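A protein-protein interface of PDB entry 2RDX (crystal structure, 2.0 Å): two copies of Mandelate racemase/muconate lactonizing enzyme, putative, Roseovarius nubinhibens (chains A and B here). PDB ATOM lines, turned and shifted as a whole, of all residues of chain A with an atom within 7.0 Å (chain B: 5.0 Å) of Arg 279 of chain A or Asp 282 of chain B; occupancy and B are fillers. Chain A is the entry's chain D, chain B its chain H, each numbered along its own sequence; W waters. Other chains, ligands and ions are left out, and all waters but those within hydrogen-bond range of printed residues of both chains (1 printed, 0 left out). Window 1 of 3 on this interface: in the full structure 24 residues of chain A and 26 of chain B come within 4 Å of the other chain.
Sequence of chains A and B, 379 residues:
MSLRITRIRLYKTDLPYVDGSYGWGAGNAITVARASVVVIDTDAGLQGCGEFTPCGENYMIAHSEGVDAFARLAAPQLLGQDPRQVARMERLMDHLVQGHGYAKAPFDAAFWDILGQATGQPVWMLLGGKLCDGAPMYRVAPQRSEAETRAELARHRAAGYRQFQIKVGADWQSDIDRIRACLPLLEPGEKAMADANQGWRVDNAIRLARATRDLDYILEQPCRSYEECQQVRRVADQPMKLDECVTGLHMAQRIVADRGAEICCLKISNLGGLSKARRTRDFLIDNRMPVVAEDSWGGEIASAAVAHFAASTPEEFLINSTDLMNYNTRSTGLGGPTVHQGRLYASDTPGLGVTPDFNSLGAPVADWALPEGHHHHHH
Among the printed residues, merely in contact across the chains: Leu 249 of chain A with Phe 283 of chain B, Leu 249 of chain A with Asp 286 of chain B, Arg 279 of chain A with Asp 282 of chain B, Asp 282 of chain A with Arg 279 of chain B and Phe 283 of chain A with Phe 283 of chain B.
Water W1 bridges O of Arg 279 of chain B (3.2 Å) and O of Arg 279 of chain A (3.5 Å).
Arg 278 of chain B touches its own counterpart, Arg 278 of chain A.
Arg 279 of chain A touches Asp 282 of chain B, and with the chains exchanged Asp 282 of chain A touches Arg 279 of chain B.
Phe 283 of chain B touches its own counterpart, Phe 283 of chain A.
Of the 7 pairs that touch across the chains among the printed residues, 4 have their exchanged pair printed and touching as well.
NE of Arg 279 of chain A lies within salt-bridge range of OD2 of Asp 286 of chain B (2.9 Å).
The guanidinium group (NH2) of Arg 278 of chain B lies close to the guanidinium group (NH2) of Arg 278 of chain A (2.9 Å).
Of the printed residues of chain B, Leu 249 of chain A touches Phe 283 and Asp 286.
Of the printed residues of chain B, Arg 278 of chain A touches Arg 278.
Arg 279 of chain A touches just these residues of chain B: Asp 282 and Asp 286.
Printed residues of chain A within 4 Å of Arg 278 of chain B: Arg 278 (2.9 Å).
Of chain A, only Arg 279 (3.5 Å) comes within 4 Å of Asp 282 of chain B.
Printed residues of chain A within 4 Å of Phe 283 of chain B: Leu 249 (3.7 Å) and Phe 283 (3.5 Å).
Leu 284 of chain B touches none of the printed residues of chain A.
The nearest residue of chain A that does not touch Asp 282 of chain B is Leu 249 of chain A (5.1 Å).
The nearest printed residue of chain B that does not touch Phe 283 of chain A is Arg 279 of chain B (5.7 Å).
The side-chain carboxylate of Glu 90 of chain A is in salt-bridge range of the guanidinium group of Arg 279 of chain A (2.7 Å).
NE of Arg 281 of chain A is in salt-bridge range of OD1 of Asp 282 of chain A, at 3.0 Å.
The side-chain carboxylate (OD2) of Asp 282 of chain B is in salt-bridge range of the guanidinium group (NE) of Arg 278 of chain B, at 3.9 Å.
The guanidinium group of Arg 281 of chain B lies within salt-bridge range of the side-chain carboxylate of Asp 282 of chain B (3.7 Å).
Printed residues of chain B that touch a printed residue of chain A: Arg 278, Arg 279, Asp 282, Phe 283 and Asp 286.
Hydrophobic or aromatic side chains of chain B within 4 Å of the printed part of chain A: Phe 283.
Along chain B the printed residues that touch a printed residue of chain A span positions 278 to 286.
Hydrophobic or aromatic side chains of chain A within 4 Å of the printed part of chain B: Leu 249 and Phe 283.
Among the printed residues, 7 pairs touch across the chains.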
ATOM      1  N   ALA A  87      28.102 -23.679  15.064  1.00  0.00           N
ATOM      2  CA  ALA A  87      26.824 -24.370  14.885  1.00  0.00           C
ATOM      3  C   ALA A  87      26.968 -25.875  14.979  1.00  0.00           C
ATOM      4  O   ALA A  87      26.012 -26.562  15.332  1.00  0.00           O
ATOM      5  CB  ALA A  87      26.163 -23.980  13.569  1.00  0.00           C
ATOM      6  N   GLU A  90      27.293 -26.246  18.844  1.00  0.00           N
ATOM      7  CA  GLU A  90      25.934 -26.090  19.358  1.00  0.00           C
ATOM      8  C   GLU A  90      25.084 -27.359  19.228  1.00  0.00           C
ATOM      9  O   GLU A  90      24.474 -27.806  20.203  1.00  0.00           O
ATOM     10  CB  GLU A  90      25.243 -24.930  18.645  1.00  0.00           C
ATOM     11  CG  GLU A  90      23.776 -24.787  19.006  1.00  0.00           C
ATOM     12  CD  GLU A  90      23.102 -23.675  18.274  1.00  0.00           C
ATOM     13  OE1 GLU A  90      23.700 -23.125  17.320  1.00  0.00           O
ATOM     14  OE2 GLU A  90      21.959 -23.351  18.653  1.00  0.00           O
ATOM     15  N   ASP A  94      23.807 -29.861  22.185  1.00  0.00           N
ATOM     16  CA  ASP A  94      22.379 -30.214  22.211  1.00  0.00           C
ATOM     17  C   ASP A  94      22.121 -31.722  22.017  1.00  0.00           C
ATOM     18  O   ASP A  94      21.100 -32.265  22.467  1.00  0.00           O
ATOM     19  CB  ASP A  94      21.611 -29.401  21.167  1.00  0.00           C
ATOM     20  CG  ASP A  94      21.565 -27.917  21.500  1.00  0.00           C
ATOM     21  OD1 ASP A  94      22.128 -27.519  22.544  1.00  0.00           O
ATOM     22  OD2 ASP A  94      20.968 -27.145  20.717  1.00  0.00           O
ATOM     23  N   LEU A 249      13.408 -19.418  21.138  1.00  0.00           N
ATOM     24  CA  LEU A 249      12.694 -19.122  19.907  1.00  0.00           C
ATOM     25  C   LEU A 249      11.202 -19.440  19.987  1.00  0.00           C
ATOM     26  O   LEU A 249      10.381 -18.666  19.489  1.00  0.00           O
ATOM     27  CB  LEU A 249      13.341 -19.860  18.718  1.00  0.00           C
ATOM     28  CG  LEU A 249      12.964 -19.354  17.323  1.00  0.00           C
ATOM     29  CD1 LEU A 249      13.612 -18.005  17.017  1.00  0.00           C
ATOM     30  CD2 LEU A 249      13.346 -20.384  16.272  1.00  0.00           C
ATOM     31  N   GLY A 273      22.960 -19.388  25.239  1.00  0.00           N
ATOM     32  CA  GLY A 273      24.230 -19.043  24.604  1.00  0.00           C
ATOM     33  C   GLY A 273      24.113 -17.970  23.532  1.00  0.00           C
ATOM     34  O   GLY A 273      23.023 -17.699  23.044  1.00  0.00           O
ATOM     35  N   LEU A 274      25.243 -17.363  23.171  1.00  0.00           N
ATOM     36  CA  LEU A 274      25.304 -16.372  22.088  1.00  0.00           C
ATOM     37  C   LEU A 274      24.744 -16.828  20.727  1.00  0.00           C
ATOM     38  O   LEU A 274      24.174 -16.017  20.006  1.00  0.00           O
ATOM     39  CB  LEU A 274      26.734 -15.851  21.925  1.00  0.00           C
ATOM     40  CG  LEU A 274      27.019 -14.630  21.041  1.00  0.00           C
ATOM     41  CD1 LEU A 274      26.041 -13.477  21.298  1.00  0.00           C
ATOM     42  CD2 LEU A 274      28.447 -14.159  21.252  1.00  0.00           C
ATOM     43  N   SER A 275      24.906 -18.102  20.382  1.00  0.00           N
ATOM     44  CA  SER A 275      24.372 -18.655  19.127  1.00  0.00           C
ATOM     45  C   SER A 275      22.840 -18.642  19.062  1.00  0.00           C
ATOM     46  O   SER A 275      22.266 -18.238  18.055  1.00  0.00           O
ATOM     47  CB  SER A 275      24.879 -20.082  18.916  1.00  0.00           C
ATOM     48  OG  SER A 275      26.277 -20.112  18.663  1.00  0.00           O
ATOM     49  N   LYS A 276      22.182 -19.097  20.128  1.00  0.00           N
ATOM     50  CA  LYS A 276      20.717 -19.084  20.183  1.00  0.00           C
ATOM     51  C   LYS A 276      20.164 -17.677  20.425  1.00  0.00           C
ATOM     52  O   LYS A 276      19.119 -17.320  19.896  1.00  0.00           O
ATOM     53  CB  LYS A 276      20.211 -20.046  21.246  1.00  0.00           C
ATOM     54  CG  LYS A 276      20.217 -21.504  20.826  1.00  0.00           C
ATOM     55  CD  LYS A 276      19.851 -22.415  21.989  1.00  0.00           C
ATOM     56  CE  LYS A 276      19.842 -23.880  21.576  1.00  0.00           C
ATOM     57  NZ  LYS A 276      21.205 -24.429  21.317  1.00  0.00           N
ATOM     58  N   ALA A 277      20.883 -16.883  21.219  1.00  0.00           N
ATOM     59  CA  ALA A 277      20.508 -15.499  21.507  1.00  0.00           C
ATOM     60  C   ALA A 277      20.467 -14.623  20.256  1.00  0.00           C
ATOM     61  O   ALA A 277      19.537 -13.821  20.077  1.00  0.00           O
ATOM     62  CB  ALA A 277      21.447 -14.902  22.554  1.00  0.00           C
ATOM     63  N   ARG A 278      21.477 -14.777  19.436  1.00  0.00           N
ATOM     64  CA  ARG A 278      21.564 -14.162  18.152  1.00  0.00           C
ATOM     65  C   ARG A 278      20.363 -14.472  17.272  1.00  0.00           C
ATOM     66  O   ARG A 278      19.777 -13.643  16.669  1.00  0.00           O
ATOM     67  CB  ARG A 278      22.850 -14.616  17.476  1.00  0.00           C
ATOM     68  CG  ARG A 278      22.948 -14.167  16.121  1.00  0.00           C
ATOM     69  CD  ARG A 278      23.462 -15.187  15.200  1.00  0.00           C
ATOM     70  NE  ARG A 278      24.190 -14.541  14.137  1.00  0.00           N
ATOM     71  CZ  ARG A 278      24.970 -15.181  13.298  1.00  0.00           C
ATOM     72  NH1 ARG A 278      25.607 -14.531  12.360  1.00  0.00           N
ATOM     73  NH2 ARG A 278      25.106 -16.480  13.407  1.00  0.00           N
ATOM     74  N   ARG A 279      20.013 -15.731  17.217  1.00  0.00           N
ATOM     75  CA  ARG A 279      18.926 -16.206  16.370  1.00  0.00           C
ATOM     76  C   ARG A 279      17.562 -15.729  16.831  1.00  0.00           C
ATOM     77  O   ARG A 279      16.689 -15.481  16.005  1.00  0.00           O
ATOM     78  CB  ARG A 279      18.961 -17.731  16.242  1.00  0.00           C
ATOM     79  CG  ARG A 279      20.174 -18.213  15.426  1.00  0.00           C
ATOM     80  CD  ARG A 279      19.937 -19.575  14.798  1.00  0.00           C
ATOM     81  NE  ARG A 279      19.555 -20.584  15.784  1.00  0.00           N
ATOM     82  CZ  ARG A 279      20.411 -21.357  16.448  1.00  0.00           C
ATOM     83  NH1 ARG A 279      21.717 -21.257  16.244  1.00  0.00           N
ATOM     84  NH2 ARG A 279      19.955 -22.240  17.321  1.00  0.00           N
ATOM     85  N   THR A 280      17.392 -15.588  18.143  1.00  0.00           N
ATOM     86  CA  THR A 280      16.147 -15.063  18.705  1.00  0.00           C
ATOM     87  C   THR A 280      16.042 -13.541  18.489  1.00  0.00           C
ATOM     88  O   THR A 280      14.958 -13.040  18.202  1.00  0.00           O
ATOM     89  CB  THR A 280      15.941 -15.497  20.189  1.00  0.00           C
ATOM     90  OG1 THR A 280      15.700 -16.908  20.240  1.00  0.00           O
ATOM     91  CG2 THR A 280      14.751 -14.815  20.817  1.00  0.00           C
ATOM     92  N   ARG A 281      17.135 -12.834  18.663  1.00  0.00           N
ATOM     93  CA  ARG A 281      17.316 -11.436  18.292  1.00  0.00           C
ATOM     94  C   ARG A 281      16.839 -11.115  16.888  1.00  0.00           C
ATOM     95  O   ARG A 281      16.022 -10.262  16.667  1.00  0.00           O
ATOM     96  CB  ARG A 281      18.807 -11.178  18.356  1.00  0.00           C
ATOM     97  CG  ARG A 281      19.247  -9.804  18.504  1.00  0.00           C
ATOM     98  CD  ARG A 281      19.708  -9.247  17.233  1.00  0.00           C
ATOM     99  NE  ARG A 281      20.906  -9.809  16.652  1.00  0.00           N
ATOM    100  CZ  ARG A 281      22.139  -9.598  17.064  1.00  0.00           C
ATOM    101  NH1 ARG A 281      23.133 -10.122  16.416  1.00  0.00           N
ATOM    102  NH2 ARG A 281      22.389  -8.877  18.115  1.00  0.00           N
ATOM    103  N   ASP A 282      17.398 -11.847  15.957  1.00  0.00           N
ATOM    104  CA  ASP A 282      17.235 -11.700  14.511  1.00  0.00           C
ATOM    105  C   ASP A 282      15.789 -11.955  14.108  1.00  0.00           C
ATOM    106  O   ASP A 282      15.245 -11.270  13.245  1.00  0.00           O
ATOM    107  CB  ASP A 282      18.140 -12.690  13.779  1.00  0.00           C
ATOM    108  CG  ASP A 282      19.571 -12.198  13.633  1.00  0.00           C
ATOM    109  OD1 ASP A 282      19.904 -11.095  14.122  1.00  0.00           O
ATOM    110  OD2 ASP A 282      20.373 -12.931  13.012  1.00  0.00           O
ATOM    111  N   PHE A 283      15.188 -12.957  14.742  1.00  0.00           N
ATOM    112  CA  PHE A 283      13.784 -13.284  14.552  1.00  0.00           C
ATOM    113  C   PHE A 283      12.884 -12.142  15.029  1.00  0.00           C
ATOM    114  O   PHE A 283      11.940 -11.750  14.341  1.00  0.00           O
ATOM    115  CB  PHE A 283      13.430 -14.569  15.308  1.00  0.00           C
ATOM    116  CG  PHE A 283      11.965 -14.856  15.328  1.00  0.00           C
ATOM    117  CD1 PHE A 283      11.354 -15.474  14.240  1.00  0.00           C
ATOM    118  CD2 PHE A 283      11.182 -14.477  16.418  1.00  0.00           C
ATOM    119  CE1 PHE A 283       9.982 -15.708  14.244  1.00  0.00           C
ATOM    120  CE2 PHE A 283       9.819 -14.715  16.430  1.00  0.00           C
ATOM    121  CZ  PHE A 283       9.217 -15.335  15.340  1.00  0.00           C
ATOM    122  N   LEU A 284      13.169 -11.640  16.226  1.00  0.00           N
ATOM    123  CA  LEU A 284      12.392 -10.546  16.814  1.00  0.00           C
ATOM    124  C   LEU A 284      12.545  -9.238  16.040  1.00  0.00           C
ATOM    125  O   LEU A 284      11.567  -8.519  15.853  1.00  0.00           O
ATOM    126  CB  LEU A 284      12.729 -10.381  18.306  1.00  0.00           C
ATOM    127  CG  LEU A 284      12.129 -11.461  19.222  1.00  0.00           C
ATOM    128  CD1 LEU A 284      12.807 -11.498  20.584  1.00  0.00           C
ATOM    129  CD2 LEU A 284      10.613 -11.292  19.373  1.00  0.00           C
ATOM    130  N   PHE A 309      26.927  -8.748  21.176  1.00  0.00           N
ATOM    131  CA  PHE A 309      25.493  -9.002  20.972  1.00  0.00           C
ATOM    132  C   PHE A 309      24.721  -7.688  20.794  1.00  0.00           C
ATOM    133  O   PHE A 309      23.901  -7.567  19.880  1.00  0.00           O
ATOM    134  CB  PHE A 309      24.963  -9.819  22.173  1.00  0.00           C
ATOM    135  CG  PHE A 309      23.527 -10.316  22.047  1.00  0.00           C
ATOM    136  CD1 PHE A 309      23.052 -10.897  20.880  1.00  0.00           C
ATOM    137  CD2 PHE A 309      22.685 -10.280  23.152  1.00  0.00           C
ATOM    138  CE1 PHE A 309      21.743 -11.380  20.806  1.00  0.00           C
ATOM    139  CE2 PHE A 309      21.365 -10.757  23.087  1.00  0.00           C
ATOM    140  CZ  PHE A 309      20.893 -11.298  21.909  1.00  0.00           C
ATOM    141  N   ALA B 277      18.105 -15.957   3.642  1.00  0.00           N
ATOM    142  CA  ALA B 277      17.953 -17.387   3.423  1.00  0.00           C
ATOM    143  C   ALA B 277      18.451 -18.176   4.634  1.00  0.00           C
ATOM    144  O   ALA B 277      17.799 -19.122   5.064  1.00  0.00           O
ATOM    145  CB  ALA B 277      18.679 -17.809   2.151  1.00  0.00           C
ATOM    146  N   ARG B 278      19.601 -17.754   5.168  1.00  0.00           N
ATOM    147  CA  ARG B 278      20.224 -18.319   6.365  1.00  0.00           C
ATOM    148  C   ARG B 278      19.319 -18.242   7.584  1.00  0.00           C
ATOM    149  O   ARG B 278      19.206 -19.195   8.361  1.00  0.00           O
ATOM    150  CB  ARG B 278      21.504 -17.547   6.692  1.00  0.00           C
ATOM    151  CG  ARG B 278      22.205 -18.063   7.906  1.00  0.00           C
ATOM    152  CD  ARG B 278      22.676 -16.968   8.814  1.00  0.00           C
ATOM    153  NE  ARG B 278      23.711 -17.526   9.669  1.00  0.00           N
ATOM    154  CZ  ARG B 278      24.811 -16.883  10.034  1.00  0.00           C
ATOM    155  NH1 ARG B 278      25.027 -15.638   9.629  1.00  0.00           N
ATOM    156  NH2 ARG B 278      25.699 -17.496  10.804  1.00  0.00           N
ATOM    157  N   ARG B 279      18.702 -17.083   7.758  1.00  0.00           N
ATOM    158  CA  ARG B 279      17.881 -16.834   8.921  1.00  0.00           C
ATOM    159  C   ARG B 279      16.562 -17.600   8.871  1.00  0.00           C
ATOM    160  O   ARG B 279      16.071 -18.052   9.903  1.00  0.00           O
ATOM    161  CB  ARG B 279      17.671 -15.337   9.102  1.00  0.00           C
ATOM    162  CG  ARG B 279      18.950 -14.632   9.558  1.00  0.00           C
ATOM    163  CD  ARG B 279      18.655 -13.278  10.174  1.00  0.00           C
ATOM    164  NE  ARG B 279      17.782 -12.473   9.326  1.00  0.00           N
ATOM    165  CZ  ARG B 279      18.207 -11.544   8.481  1.00  0.00           C
ATOM    166  NH1 ARG B 279      19.502 -11.273   8.381  1.00  0.00           N
ATOM    167  NH2 ARG B 279      17.329 -10.871   7.749  1.00  0.00           N
ATOM    168  N   THR B 280      16.017 -17.760   7.666  1.00  0.00           N
ATOM    169  CA  THR B 280      14.806 -18.551   7.450  1.00  0.00           C
ATOM    170  C   THR B 280      15.125 -20.046   7.602  1.00  0.00           C
ATOM    171  O   THR B 280      14.339 -20.798   8.174  1.00  0.00           O
ATOM    172  CB  THR B 280      14.150 -18.194   6.092  1.00  0.00           C
ATOM    173  OG1 THR B 280      13.606 -16.875   6.171  1.00  0.00           O
ATOM    174  CG2 THR B 280      13.025 -19.141   5.730  1.00  0.00           C
ATOM    175  N   ARG B 281      16.306 -20.449   7.130  1.00  0.00           N
ATOM    176  CA  ARG B 281      16.798 -21.817   7.303  1.00  0.00           C
ATOM    177  C   ARG B 281      16.953 -22.194   8.769  1.00  0.00           C
ATOM    178  O   ARG B 281      16.480 -23.250   9.194  1.00  0.00           O
ATOM    179  CB  ARG B 281      18.133 -22.012   6.564  1.00  0.00           C
ATOM    180  CG  ARG B 281      18.652 -23.439   6.546  1.00  0.00           C
ATOM    181  CD  ARG B 281      19.865 -23.643   7.431  1.00  0.00           C
ATOM    182  NE  ARG B 281      21.096 -23.259   6.763  1.00  0.00           N
ATOM    183  CZ  ARG B 281      21.983 -22.420   7.273  1.00  0.00           C
ATOM    184  NH1 ARG B 281      21.792 -21.883   8.461  1.00  0.00           N
ATOM    185  NH2 ARG B 281      23.070 -22.123   6.598  1.00  0.00           N
ATOM    186  N   ASP B 282      17.625 -21.328   9.524  1.00  0.00           N
ATOM    187  CA  ASP B 282      17.882 -21.541  10.943  1.00  0.00           C
ATOM    188  C   ASP B 282      16.597 -21.584  11.764  1.00  0.00           C
ATOM    189  O   ASP B 282      16.500 -22.352  12.727  1.00  0.00           O
ATOM    190  CB  ASP B 282      18.819 -20.454  11.482  1.00  0.00           C
ATOM    191  CG  ASP B 282      20.279 -20.678  11.091  1.00  0.00           C
ATOM    192  OD1 ASP B 282      20.575 -21.656  10.374  1.00  0.00           O
ATOM    193  OD2 ASP B 282      21.141 -19.877  11.508  1.00  0.00           O
ATOM    194  N   PHE B 283      15.620 -20.764  11.371  1.00  0.00           N
ATOM    195  CA  PHE B 283      14.294 -20.742  11.991  1.00  0.00           C
ATOM    196  C   PHE B 283      13.534 -22.050  11.794  1.00  0.00           C
ATOM    197  O   PHE B 283      12.953 -22.577  12.737  1.00  0.00           O
ATOM    198  CB  PHE B 283      13.462 -19.576  11.432  1.00  0.00           C
ATOM    199  CG  PHE B 283      12.034 -19.557  11.910  1.00  0.00           C
ATOM    200  CD1 PHE B 283      11.721 -19.092  13.182  1.00  0.00           C
ATOM    201  CD2 PHE B 283      10.997 -19.985  11.079  1.00  0.00           C
ATOM    202  CE1 PHE B 283      10.402 -19.092  13.637  1.00  0.00           C
ATOM    203  CE2 PHE B 283       9.676 -19.973  11.525  1.00  0.00           C
ATOM    204  CZ  PHE B 283       9.381 -19.519  12.809  1.00  0.00           C
ATOM    205  N   LEU B 284      13.522 -22.550  10.562  1.00  0.00           N
ATOM    206  CA  LEU B 284      12.791 -23.776  10.236  1.00  0.00           C
ATOM    207  C   LEU B 284      13.398 -25.007  10.893  1.00  0.00           C
ATOM    208  O   LEU B 284      12.671 -25.871  11.373  1.00  0.00           O
ATOM    209  CB  LEU B 284      12.690 -23.965   8.720  1.00  0.00           C
ATOM    210  CG  LEU B 284      11.739 -23.017   7.991  1.00  0.00           C
ATOM    211  CD1 LEU B 284      11.973 -23.093   6.493  1.00  0.00           C
ATOM    212  CD2 LEU B 284      10.299 -23.350   8.332  1.00  0.00           C
ATOM    213  N   ILE B 285      14.727 -25.068  10.919  1.00  0.00           N
ATOM    214  CA  ILE B 285      15.466 -26.153  11.579  1.00  0.00           C
ATOM    215  C   ILE B 285      15.262 -26.172  13.103  1.00  0.00           C
ATOM    216  O   ILE B 285      15.030 -27.230  13.678  1.00  0.00           O
ATOM    217  CB  ILE B 285      16.964 -26.142  11.155  1.00  0.00           C
ATOM    218  CG1 ILE B 285      17.140 -27.031   9.927  1.00  0.00           C
ATOM    219  CG2 ILE B 285      17.881 -26.647  12.263  1.00  0.00           C
ATOM    220  CD1 ILE B 285      17.854 -26.378   8.835  1.00  0.00           C
ATOM    221  N   ASP B 286      15.274 -24.996  13.732  1.00  0.00           N
ATOM    222  CA  ASP B 286      14.950 -24.872  15.159  1.00  0.00           C
ATOM    223  C   ASP B 286      13.517 -25.290  15.478  1.00  0.00           C
ATOM    224  O   ASP B 286      13.187 -25.604  16.627  1.00  0.00           O
ATOM    225  CB  ASP B 286      15.218 -23.451  15.659  1.00  0.00           C
ATOM    226  CG  ASP B 286      16.699 -23.191  15.950  1.00  0.00           C
ATOM    227  OD1 ASP B 286      17.501 -24.157  15.953  1.00  0.00           O
ATOM    228  OD2 ASP B 286      17.056 -22.012  16.174  1.00  0.00           O
HETATM  229  O   HOH W   1      16.633 -16.619  12.723  1.00  0.00           O
